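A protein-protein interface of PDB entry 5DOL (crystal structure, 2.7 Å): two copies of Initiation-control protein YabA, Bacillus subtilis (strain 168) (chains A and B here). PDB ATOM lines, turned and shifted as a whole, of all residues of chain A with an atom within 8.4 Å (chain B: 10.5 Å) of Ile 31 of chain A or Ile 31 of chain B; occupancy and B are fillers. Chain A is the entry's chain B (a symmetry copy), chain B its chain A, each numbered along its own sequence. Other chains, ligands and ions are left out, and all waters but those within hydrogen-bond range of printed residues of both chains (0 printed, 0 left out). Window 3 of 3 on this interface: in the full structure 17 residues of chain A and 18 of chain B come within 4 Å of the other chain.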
ATOM      1  N   LEU A  24      28.727 -11.479  26.755  1.00  0.00           N
ATOM      2  CA  LEU A  24      27.959 -10.566  25.932  1.00  0.00           C
ATOM      3  C   LEU A  24      28.087 -10.959  24.471  1.00  0.00           C
ATOM      4  O   LEU A  24      27.123 -10.863  23.704  1.00  0.00           O
ATOM      5  CB  LEU A  24      28.435  -9.131  26.148  1.00  0.00           C
ATOM      6  CG  LEU A  24      27.366  -8.051  26.304  1.00  0.00           C
ATOM      7  CD1 LEU A  24      26.358  -8.451  27.367  1.00  0.00           C
ATOM      8  CD2 LEU A  24      28.028  -6.735  26.673  1.00  0.00           C
ATOM      9  N   GLY A  25      29.283 -11.399  24.084  1.00  0.00           N
ATOM     10  CA  GLY A  25      29.486 -11.895  22.728  1.00  0.00           C
ATOM     11  C   GLY A  25      28.637 -13.119  22.394  1.00  0.00           C
ATOM     12  O   GLY A  25      27.944 -13.168  21.354  1.00  0.00           O
ATOM     13  N   ASP A  26      28.682 -14.115  23.277  1.00  0.00           N
ATOM     14  CA  ASP A  26      27.884 -15.323  23.068  1.00  0.00           C
ATOM     15  C   ASP A  26      26.398 -14.985  23.011  1.00  0.00           C
ATOM     16  O   ASP A  26      25.656 -15.481  22.142  1.00  0.00           O
ATOM     17  CB  ASP A  26      28.155 -16.350  24.165  1.00  0.00           C
ATOM     18  CG  ASP A  26      29.341 -17.237  23.843  1.00  0.00           C
ATOM     19  OD1 ASP A  26      29.140 -18.274  23.173  1.00  0.00           O
ATOM     20  OD2 ASP A  26      30.471 -16.895  24.252  1.00  0.00           O
ATOM     21  N   LEU A  27      25.979 -14.124  23.936  1.00  0.00           N
ATOM     22  CA  LEU A  27      24.616 -13.619  23.944  1.00  0.00           C
ATOM     23  C   LEU A  27      24.259 -13.045  22.577  1.00  0.00           C
ATOM     24  O   LEU A  27      23.222 -13.388  22.018  1.00  0.00           O
ATOM     25  CB  LEU A  27      24.432 -12.559  25.030  1.00  0.00           C
ATOM     26  CG  LEU A  27      22.991 -12.089  25.244  1.00  0.00           C
ATOM     27  CD1 LEU A  27      22.129 -13.228  25.765  1.00  0.00           C
ATOM     28  CD2 LEU A  27      22.944 -10.899  26.191  1.00  0.00           C
ATOM     29  N   LYS A  28      25.129 -12.192  22.037  1.00  0.00           N
ATOM     30  CA  LYS A  28      24.922 -11.622  20.707  1.00  0.00           C
ATOM     31  C   LYS A  28      24.696 -12.709  19.655  1.00  0.00           C
ATOM     32  O   LYS A  28      23.774 -12.620  18.824  1.00  0.00           O
ATOM     33  CB  LYS A  28      26.115 -10.755  20.292  1.00  0.00           C
ATOM     34  CG  LYS A  28      25.952 -10.114  18.922  1.00  0.00           C
ATOM     35  CD  LYS A  28      27.290  -9.760  18.292  1.00  0.00           C
ATOM     36  CE  LYS A  28      28.051  -8.742  19.125  1.00  0.00           C
ATOM     37  NZ  LYS A  28      29.340  -8.359  18.485  1.00  0.00           N
ATOM     38  N   GLN A  29      25.544 -13.736  19.699  1.00  0.00           N
ATOM     39  CA  GLN A  29      25.411 -14.849  18.760  1.00  0.00           C
ATOM     40  C   GLN A  29      24.029 -15.523  18.836  1.00  0.00           C
ATOM     41  O   GLN A  29      23.328 -15.678  17.816  1.00  0.00           O
ATOM     42  CB  GLN A  29      26.509 -15.877  19.015  1.00  0.00           C
ATOM     43  CG  GLN A  29      26.365 -17.149  18.210  1.00  0.00           C
ATOM     44  CD  GLN A  29      27.368 -18.198  18.635  1.00  0.00           C
ATOM     45  OE1 GLN A  29      28.296 -17.913  19.393  1.00  0.00           O
ATOM     46  NE2 GLN A  29      27.186 -19.421  18.153  1.00  0.00           N
ATOM     47  N   HIS A  30      23.640 -15.915  20.047  1.00  0.00           N
ATOM     48  CA  HIS A  30      22.349 -16.572  20.243  1.00  0.00           C
ATOM     49  C   HIS A  30      21.189 -15.670  19.817  1.00  0.00           C
ATOM     50  O   HIS A  30      20.195 -16.137  19.256  1.00  0.00           O
ATOM     51  CB  HIS A  30      22.183 -16.999  21.705  1.00  0.00           C
ATOM     52  CG  HIS A  30      23.170 -18.035  22.150  1.00  0.00           C
ATOM     53  ND1 HIS A  30      23.967 -18.732  21.267  1.00  0.00           N
ATOM     54  CD2 HIS A  30      23.489 -18.489  23.385  1.00  0.00           C
ATOM     55  CE1 HIS A  30      24.735 -19.571  21.939  1.00  0.00           C
ATOM     56  NE2 HIS A  30      24.465 -19.443  23.226  1.00  0.00           N
ATOM     57  N   ILE A  31      21.329 -14.375  20.083  1.00  0.00           N
ATOM     58  CA  ILE A  31      20.323 -13.394  19.700  1.00  0.00           C
ATOM     59  C   ILE A  31      20.138 -13.376  18.187  1.00  0.00           C
ATOM     60  O   ILE A  31      19.012 -13.493  17.687  1.00  0.00           O
ATOM     61  CB  ILE A  31      20.694 -11.982  20.189  1.00  0.00           C
ATOM     62  CG1 ILE A  31      20.484 -11.877  21.694  1.00  0.00           C
ATOM     63  CG2 ILE A  31      19.850 -10.929  19.480  1.00  0.00           C
ATOM     64  CD1 ILE A  31      19.108 -12.284  22.119  1.00  0.00           C
ATOM     65  N   GLY A  32      21.245 -13.234  17.463  1.00  0.00           N
ATOM     66  CA  GLY A  32      21.197 -13.288  16.012  1.00  0.00           C
ATOM     67  C   GLY A  32      20.528 -14.558  15.518  1.00  0.00           C
ATOM     68  O   GLY A  32      19.669 -14.523  14.616  1.00  0.00           O
ATOM     69  N   GLU A  33      20.911 -15.683  16.123  1.00  0.00           N
ATOM     70  CA  GLU A  33      20.290 -16.965  15.788  1.00  0.00           C
ATOM     71  C   GLU A  33      18.764 -16.911  15.922  1.00  0.00           C
ATOM     72  O   GLU A  33      18.035 -17.242  14.979  1.00  0.00           O
ATOM     73  CB  GLU A  33      20.869 -18.081  16.662  1.00  0.00           C
ATOM     74  CG  GLU A  33      22.324 -18.396  16.336  1.00  0.00           C
ATOM     75  CD  GLU A  33      22.946 -19.385  17.299  1.00  0.00           C
ATOM     76  OE1 GLU A  33      22.269 -19.775  18.276  1.00  0.00           O
ATOM     77  OE2 GLU A  33      24.115 -19.772  17.083  1.00  0.00           O
ATOM     78  N   MET A  34      18.282 -16.466  17.080  1.00  0.00           N
ATOM     79  CA  MET A  34      16.846 -16.332  17.300  1.00  0.00           C
ATOM     80  C   MET A  34      16.180 -15.383  16.295  1.00  0.00           C
ATOM     81  O   MET A  34      15.031 -15.590  15.905  1.00  0.00           O
ATOM     82  CB  MET A  34      16.573 -15.857  18.724  1.00  0.00           C
ATOM     83  CG  MET A  34      15.091 -15.795  19.088  1.00  0.00           C
ATOM     84  SD  MET A  34      14.854 -15.157  20.756  1.00  0.00           S
ATOM     85  CE  MET A  34      15.839 -16.329  21.682  1.00  0.00           C
ATOM     86  N   ILE A  35      16.899 -14.349  15.868  1.00  0.00           N
ATOM     87  CA  ILE A  35      16.347 -13.403  14.897  1.00  0.00           C
ATOM     88  C   ILE A  35      16.142 -14.072  13.537  1.00  0.00           C
ATOM     89  O   ILE A  35      15.079 -13.929  12.900  1.00  0.00           O
ATOM     90  CB  ILE A  35      17.256 -12.163  14.736  1.00  0.00           C
ATOM     91  CG1 ILE A  35      17.318 -11.380  16.049  1.00  0.00           C
ATOM     92  CG2 ILE A  35      16.751 -11.266  13.617  1.00  0.00           C
ATOM     93  CD1 ILE A  35      18.204 -10.160  16.006  1.00  0.00           C
ATOM     94  N   GLU A  36      17.162 -14.811  13.103  1.00  0.00           N
ATOM     95  CA  GLU A  36      17.054 -15.579  11.866  1.00  0.00           C
ATOM     96  C   GLU A  36      15.888 -16.566  11.961  1.00  0.00           C
ATOM     97  O   GLU A  36      15.058 -16.655  11.048  1.00  0.00           O
ATOM     98  CB  GLU A  36      18.361 -16.325  11.565  1.00  0.00           C
ATOM     99  CG  GLU A  36      19.540 -15.418  11.244  1.00  0.00           C
ATOM    100  CD  GLU A  36      20.784 -16.188  10.825  1.00  0.00           C
ATOM    101  OE1 GLU A  36      20.770 -17.437  10.894  1.00  0.00           O
ATOM    102  OE2 GLU A  36      21.776 -15.543  10.420  1.00  0.00           O
ATOM    103  N   GLU A  37      15.824 -17.289  13.078  1.00  0.00           N
ATOM    104  CA  GLU A  37      14.745 -18.249  13.307  1.00  0.00           C
ATOM    105  C   GLU A  37      13.377 -17.583  13.158  1.00  0.00           C
ATOM    106  O   GLU A  37      12.485 -18.106  12.472  1.00  0.00           O
ATOM    107  CB  GLU A  37      14.876 -18.889  14.691  1.00  0.00           C
ATOM    108  CG  GLU A  37      13.925 -20.049  14.923  1.00  0.00           C
ATOM    109  CD  GLU A  37      14.239 -20.824  16.192  1.00  0.00           C
ATOM    110  OE1 GLU A  37      15.074 -20.347  16.992  1.00  0.00           O
ATOM    111  OE2 GLU A  37      13.652 -21.913  16.386  1.00  0.00           O
ATOM    112  N   ASN A  38      13.226 -16.418  13.787  1.00  0.00           N
ATOM    113  CA  ASN A  38      11.993 -15.649  13.677  1.00  0.00           C
ATOM    114  C   ASN A  38      11.662 -15.268  12.230  1.00  0.00           C
ATOM    115  O   ASN A  38      10.510 -15.402  11.808  1.00  0.00           O
ATOM    116  CB  ASN A  38      12.060 -14.396  14.552  1.00  0.00           C
ATOM    117  CG  ASN A  38      11.524 -14.634  15.957  1.00  0.00           C
ATOM    118  OD1 ASN A  38      11.451 -15.772  16.425  1.00  0.00           O
ATOM    119  ND2 ASN A  38      11.142 -13.556  16.634  1.00  0.00           N
ATOM    120  N   GLN B  23      20.570  -0.509  30.793  1.00  0.00           N
ATOM    121  CA  GLN B  23      20.568  -0.886  29.377  1.00  0.00           C
ATOM    122  C   GLN B  23      20.346  -2.393  29.161  1.00  0.00           C
ATOM    123  O   GLN B  23      19.657  -2.818  28.220  1.00  0.00           O
ATOM    124  CB  GLN B  23      21.878  -0.451  28.720  1.00  0.00           C
ATOM    125  CG  GLN B  23      22.041   1.051  28.641  1.00  0.00           C
ATOM    126  CD  GLN B  23      23.321   1.463  27.937  1.00  0.00           C
ATOM    127  OE1 GLN B  23      23.645   0.957  26.862  1.00  0.00           O
ATOM    128  NE2 GLN B  23      24.061   2.383  28.546  1.00  0.00           N
ATOM    129  N   LEU B  24      20.935  -3.191  30.043  1.00  0.00           N
ATOM    130  CA  LEU B  24      20.817  -4.637  29.977  1.00  0.00           C
ATOM    131  C   LEU B  24      19.406  -5.055  30.355  1.00  0.00           C
ATOM    132  O   LEU B  24      18.911  -6.082  29.892  1.00  0.00           O
ATOM    133  CB  LEU B  24      21.841  -5.308  30.895  1.00  0.00           C
ATOM    134  CG  LEU B  24      21.870  -6.835  30.873  1.00  0.00           C
ATOM    135  CD1 LEU B  24      22.177  -7.347  29.479  1.00  0.00           C
ATOM    136  CD2 LEU B  24      22.877  -7.364  31.866  1.00  0.00           C
ATOM    137  N   GLY B  25      18.761  -4.257  31.202  1.00  0.00           N
ATOM    138  CA  GLY B  25      17.363  -4.482  31.534  1.00  0.00           C
ATOM    139  C   GLY B  25      16.481  -4.267  30.316  1.00  0.00           C
ATOM    140  O   GLY B  25      15.601  -5.093  30.006  1.00  0.00           O
ATOM    141  N   ASP B  26      16.718  -3.159  29.613  1.00  0.00           N
ATOM    142  CA  ASP B  26      15.987  -2.910  28.366  1.00  0.00           C
ATOM    143  C   ASP B  26      16.171  -4.076  27.391  1.00  0.00           C
ATOM    144  O   ASP B  26      15.190  -4.653  26.867  1.00  0.00           O
ATOM    145  CB  ASP B  26      16.448  -1.604  27.714  1.00  0.00           C
ATOM    146  CG  ASP B  26      16.257  -0.399  28.619  1.00  0.00           C
ATOM    147  OD1 ASP B  26      15.319  -0.417  29.446  1.00  0.00           O
ATOM    148  OD2 ASP B  26      17.044   0.564  28.499  1.00  0.00           O
ATOM    149  N   LEU B  27      17.438  -4.422  27.169  1.00  0.00           N
ATOM    150  CA  LEU B  27      17.779  -5.565  26.330  1.00  0.00           C
ATOM    151  C   LEU B  27      17.003  -6.820  26.738  1.00  0.00           C
ATOM    152  O   LEU B  27      16.471  -7.517  25.886  1.00  0.00           O
ATOM    153  CB  LEU B  27      19.277  -5.852  26.390  1.00  0.00           C
ATOM    154  CG  LEU B  27      19.767  -6.882  25.369  1.00  0.00           C
ATOM    155  CD1 LEU B  27      19.717  -6.289  23.969  1.00  0.00           C
ATOM    156  CD2 LEU B  27      21.174  -7.375  25.701  1.00  0.00           C
ATOM    157  N   LYS B  28      16.937  -7.092  28.040  1.00  0.00           N
ATOM    158  CA  LYS B  28      16.227  -8.260  28.549  1.00  0.00           C
ATOM    159  C   LYS B  28      14.766  -8.207  28.153  1.00  0.00           C
ATOM    160  O   LYS B  28      14.183  -9.210  27.731  1.00  0.00           O
ATOM    161  CB  LYS B  28      16.344  -8.358  30.072  1.00  0.00           C
ATOM    162  CG  LYS B  28      15.603  -9.550  30.667  1.00  0.00           C
ATOM    163  CD  LYS B  28      15.800  -9.659  32.167  1.00  0.00           C
ATOM    164  CE  LYS B  28      15.177  -8.474  32.900  1.00  0.00           C
ATOM    165  N   GLN B  29      14.175  -7.027  28.288  1.00  0.00           N
ATOM    166  CA  GLN B  29      12.791  -6.845  27.872  1.00  0.00           C
ATOM    167  C   GLN B  29      12.582  -7.196  26.392  1.00  0.00           C
ATOM    168  O   GLN B  29      11.724  -8.030  26.046  1.00  0.00           O
ATOM    169  CB  GLN B  29      12.356  -5.405  28.142  1.00  0.00           C
ATOM    170  CG  GLN B  29      10.908  -5.101  27.826  1.00  0.00           C
ATOM    171  CD  GLN B  29      10.549  -3.668  28.166  1.00  0.00           C
ATOM    172  OE1 GLN B  29      10.529  -2.796  27.295  1.00  0.00           O
ATOM    173  NE2 GLN B  29      10.274  -3.412  29.441  1.00  0.00           N
ATOM    174  N   HIS B  30      13.378  -6.580  25.519  1.00  0.00           N
ATOM    175  CA  HIS B  30      13.231  -6.794  24.079  1.00  0.00           C
ATOM    176  C   HIS B  30      13.482  -8.253  23.686  1.00  0.00           C
ATOM    177  O   HIS B  30      12.832  -8.801  22.776  1.00  0.00           O
ATOM    178  CB  HIS B  30      14.172  -5.868  23.310  1.00  0.00           C
ATOM    179  CG  HIS B  30      13.750  -4.433  23.330  1.00  0.00           C
ATOM    180  ND1 HIS B  30      13.749  -3.673  24.482  1.00  0.00           N
ATOM    181  CD2 HIS B  30      13.305  -3.617  22.345  1.00  0.00           C
ATOM    182  CE1 HIS B  30      13.328  -2.454  24.203  1.00  0.00           C
ATOM    183  NE2 HIS B  30      13.050  -2.393  22.912  1.00  0.00           N
ATOM    184  N   ILE B  31      14.432  -8.878  24.375  1.00  0.00           N
ATOM    185  CA  ILE B  31      14.763 -10.282  24.162  1.00  0.00           C
ATOM    186  C   ILE B  31      13.571 -11.154  24.537  1.00  0.00           C
ATOM    187  O   ILE B  31      13.235 -12.108  23.831  1.00  0.00           O
ATOM    188  CB  ILE B  31      16.007 -10.701  24.986  1.00  0.00           C
ATOM    189  CG1 ILE B  31      17.279 -10.165  24.330  1.00  0.00           C
ATOM    190  CG2 ILE B  31      16.090 -12.219  25.129  1.00  0.00           C
ATOM    191  CD1 ILE B  31      18.536 -10.423  25.139  1.00  0.00           C
ATOM    192  N   GLY B  32      12.927 -10.812  25.649  1.00  0.00           N
ATOM    193  CA  GLY B  32      11.721 -11.502  26.065  1.00  0.00           C
ATOM    194  C   GLY B  32      10.629 -11.406  25.010  1.00  0.00           C
ATOM    195  O   GLY B  32      10.029 -12.417  24.618  1.00  0.00           O
ATOM    196  N   GLU B  33      10.372 -10.185  24.546  1.00  0.00           N
ATOM    197  CA  GLU B  33       9.381  -9.980  23.491  1.00  0.00           C
ATOM    198  C   GLU B  33       9.684 -10.839  22.259  1.00  0.00           C
ATOM    199  O   GLU B  33       8.792 -11.490  21.702  1.00  0.00           O
ATOM    200  CB  GLU B  33       9.317  -8.505  23.101  1.00  0.00           C
ATOM    201  CG  GLU B  33       8.909  -7.589  24.244  1.00  0.00           C
ATOM    202  CD  GLU B  33       8.978  -6.124  23.867  1.00  0.00           C
ATOM    203  OE1 GLU B  33       9.502  -5.815  22.776  1.00  0.00           O
ATOM    204  OE2 GLU B  33       8.510  -5.282  24.661  1.00  0.00           O
ATOM    205  N   MET B  34      10.947 -10.858  21.847  1.00  0.00           N
ATOM    206  CA  MET B  34      11.347 -11.678  20.708  1.00  0.00           C
ATOM    207  C   MET B  34      11.141 -13.178  20.969  1.00  0.00           C
ATOM    208  O   MET B  34      10.785 -13.938  20.065  1.00  0.00           O
ATOM    209  CB  MET B  34      12.807 -11.398  20.354  1.00  0.00           C
ATOM    210  CG  MET B  34      13.344 -12.219  19.197  1.00  0.00           C
ATOM    211  SD  MET B  34      14.989 -11.666  18.714  1.00  0.00           S
ATOM    212  CE  MET B  34      14.600 -10.038  18.073  1.00  0.00           C
ATOM    213  N   ILE B  35      11.361 -13.604  22.208  1.00  0.00           N
ATOM    214  CA  ILE B  35      11.190 -15.013  22.567  1.00  0.00           C
ATOM    215  C   ILE B  35       9.728 -15.423  22.476  1.00  0.00           C
ATOM    216  O   ILE B  35       9.398 -16.472  21.908  1.00  0.00           O
ATOM    217  CB  ILE B  35      11.708 -15.306  23.988  1.00  0.00           C
ATOM    218  CG1 ILE B  35      13.235 -15.322  24.006  1.00  0.00           C
ATOM    219  CG2 ILE B  35      11.182 -16.634  24.490  1.00  0.00           C
ATOM    220  CD1 ILE B  35      13.820 -15.455  25.394  1.00  0.00           C
ATOM    221  N   GLU B  36       8.851 -14.595  23.039  1.00  0.00           N
ATOM    222  CA  GLU B  36       7.420 -14.872  22.960  1.00  0.00           C
ATOM    223  C   GLU B  36       6.966 -14.873  21.496  1.00  0.00           C
ATOM    224  O   GLU B  36       6.159 -15.721  21.078  1.00  0.00           O
ATOM    225  CB  GLU B  36       6.613 -13.852  23.773  1.00  0.00           C
ATOM    226  N   GLU B  37       7.501 -13.925  20.724  1.00  0.00           N
ATOM    227  CA  GLU B  37       7.212 -13.843  19.294  1.00  0.00           C
ATOM    228  C   GLU B  37       7.541 -15.172  18.623  1.00  0.00           C
ATOM    229  O   GLU B  37       6.714 -15.758  17.903  1.00  0.00           O
ATOM    230  CB  GLU B  37       8.003 -12.700  18.649  1.00  0.00           C
ATOM    231  CG  GLU B  37       7.696 -12.500  17.171  1.00  0.00           C
ATOM    232  N   ASN B  38       8.758 -15.641  18.882  1.00  0.00           N
ATOM    233  CA  ASN B  38       9.205 -16.952  18.436  1.00  0.00           C
ATOM    234  C   ASN B  38       8.217 -18.060  18.794  1.00  0.00           C
ATOM    235  O   ASN B  38       7.815 -18.847  17.936  1.00  0.00           O
ATOM    236  CB  ASN B  38      10.570 -17.269  19.042  1.00  0.00           C
ATOM    237  CG  ASN B  38      11.192 -18.512  18.448  1.00  0.00           C
ATOM    238  OD1 ASN B  38      11.017 -19.621  18.961  1.00  0.00           O
ATOM    239  ND2 ASN B  38      11.931 -18.334  17.360  1.00  0.00           N
ATOM    240  N   HIS B  39       7.842 -18.113  20.068  1.00  0.00           N
ATOM    241  CA  HIS B  39       6.907 -19.107  20.568  1.00  0.00           C
ATOM    242  C   HIS B  39       5.617 -19.138  19.746  1.00  0.00           C
ATOM    243  O   HIS B  39       5.209 -20.194  19.217  1.00  0.00           O
ATOM    244  CB  HIS B  39       6.598 -18.823  22.043  1.00  0.00           C
ATOM    245  CG  HIS B  39       5.663 -19.807  22.669  1.00  0.00           C
ATOM    246  ND1 HIS B  39       5.919 -21.161  22.704  1.00  0.00           N
ATOM    247  CD2 HIS B  39       4.464 -19.635  23.276  1.00  0.00           C
ATOM    248  CE1 HIS B  39       4.921 -21.781  23.311  1.00  0.00           C
ATOM    249  NE2 HIS B  39       4.025 -20.876  23.667  1.00  0.00           N
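Among the printed residues, merely in contact across the chains: Leu 27 of chain A with Leu 27 of chain B (3.97 Å), Ile 31 of chain A with Ile 31 of chain B (3.6 Å), Met 34 of chain A with Met 34 of chain B (3.7 Å), Met 34 of chain A with Ile 35 of chain B (3.6 Å), Ile 35 of chain A with Met 34 of chain B (3.6 Å), Glu 37 of chain A with Asn 38 of chain B (3.6 Å) and Asn 38 of chain A with Glu 37 of chain B (3.6 Å).
Leu 27 of chain A touches its own counterpart, Leu 27 of chain B. Glu 37 of chain A touches Asn 38 of chain B, and with the chains exchanged Asn 38 of chain A touches Glu 37 of chain B. Asn 38 of chain A touches Met 34 of chain B, but with the chains exchanged Met 34 of chain A does not touch Asn 38 of chain B (4.4 Å). Asn 38 of chain A touches its own counterpart, Asn 38 of chain B.
ND2 of Asn 38 of chain A lies within hydrogen-bond range of O of Met 34 of chain B. ND2 of Asn 38 of chain B sits at hydrogen-bond distance from OD1 of Asn 38 of chain A.
Asp 26 of chain A touches none of the printed residues of chain B. Ile 31 of chain A touches one residue of chain B. No residue of chain B comes within 4 Å of Gly 32 of chain A. Of chain B, only Met 34 and Ile 35 come within 4 Å of Met 34 of chain A. Printed residues of chain B within 4 Å of Asn 38 of chain A: Met 34, Glu 37 and Asn 38. Leu 24 of chain B touches none of the printed residues of chain A. Of the printed residues of chain A, Leu 27 of chain B touches Leu 27 (3.97 Å). Of chain A, only Ile 31 comes within 4 Å of Ile 31 of chain B. No residue of chain A comes within 4 Å of Gly 32 of chain B. Of the printed residues of chain A, Met 34 of chain B touches Met 34 (3.7 Å), Ile 35 (3.6 Å) and Asn 38 (3.5 Å). Of the printed residues of chain A, Asn 38 of chain B touches Glu 37 and Asn 38. The nearest residue of chain B that does not touch Ile 31 of chain A is Met 34 of chain B (4.5 Å).
Of the 15 printed residues of chain A, 6 touch a printed residue of chain B. Hydrophobic or aromatic side chains of chain A within 4 Å of the printed part of chain B: Leu 27, Ile 31, Met 34 and Ile 35. Among the printed residues, 9 pairs touch across the chains.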
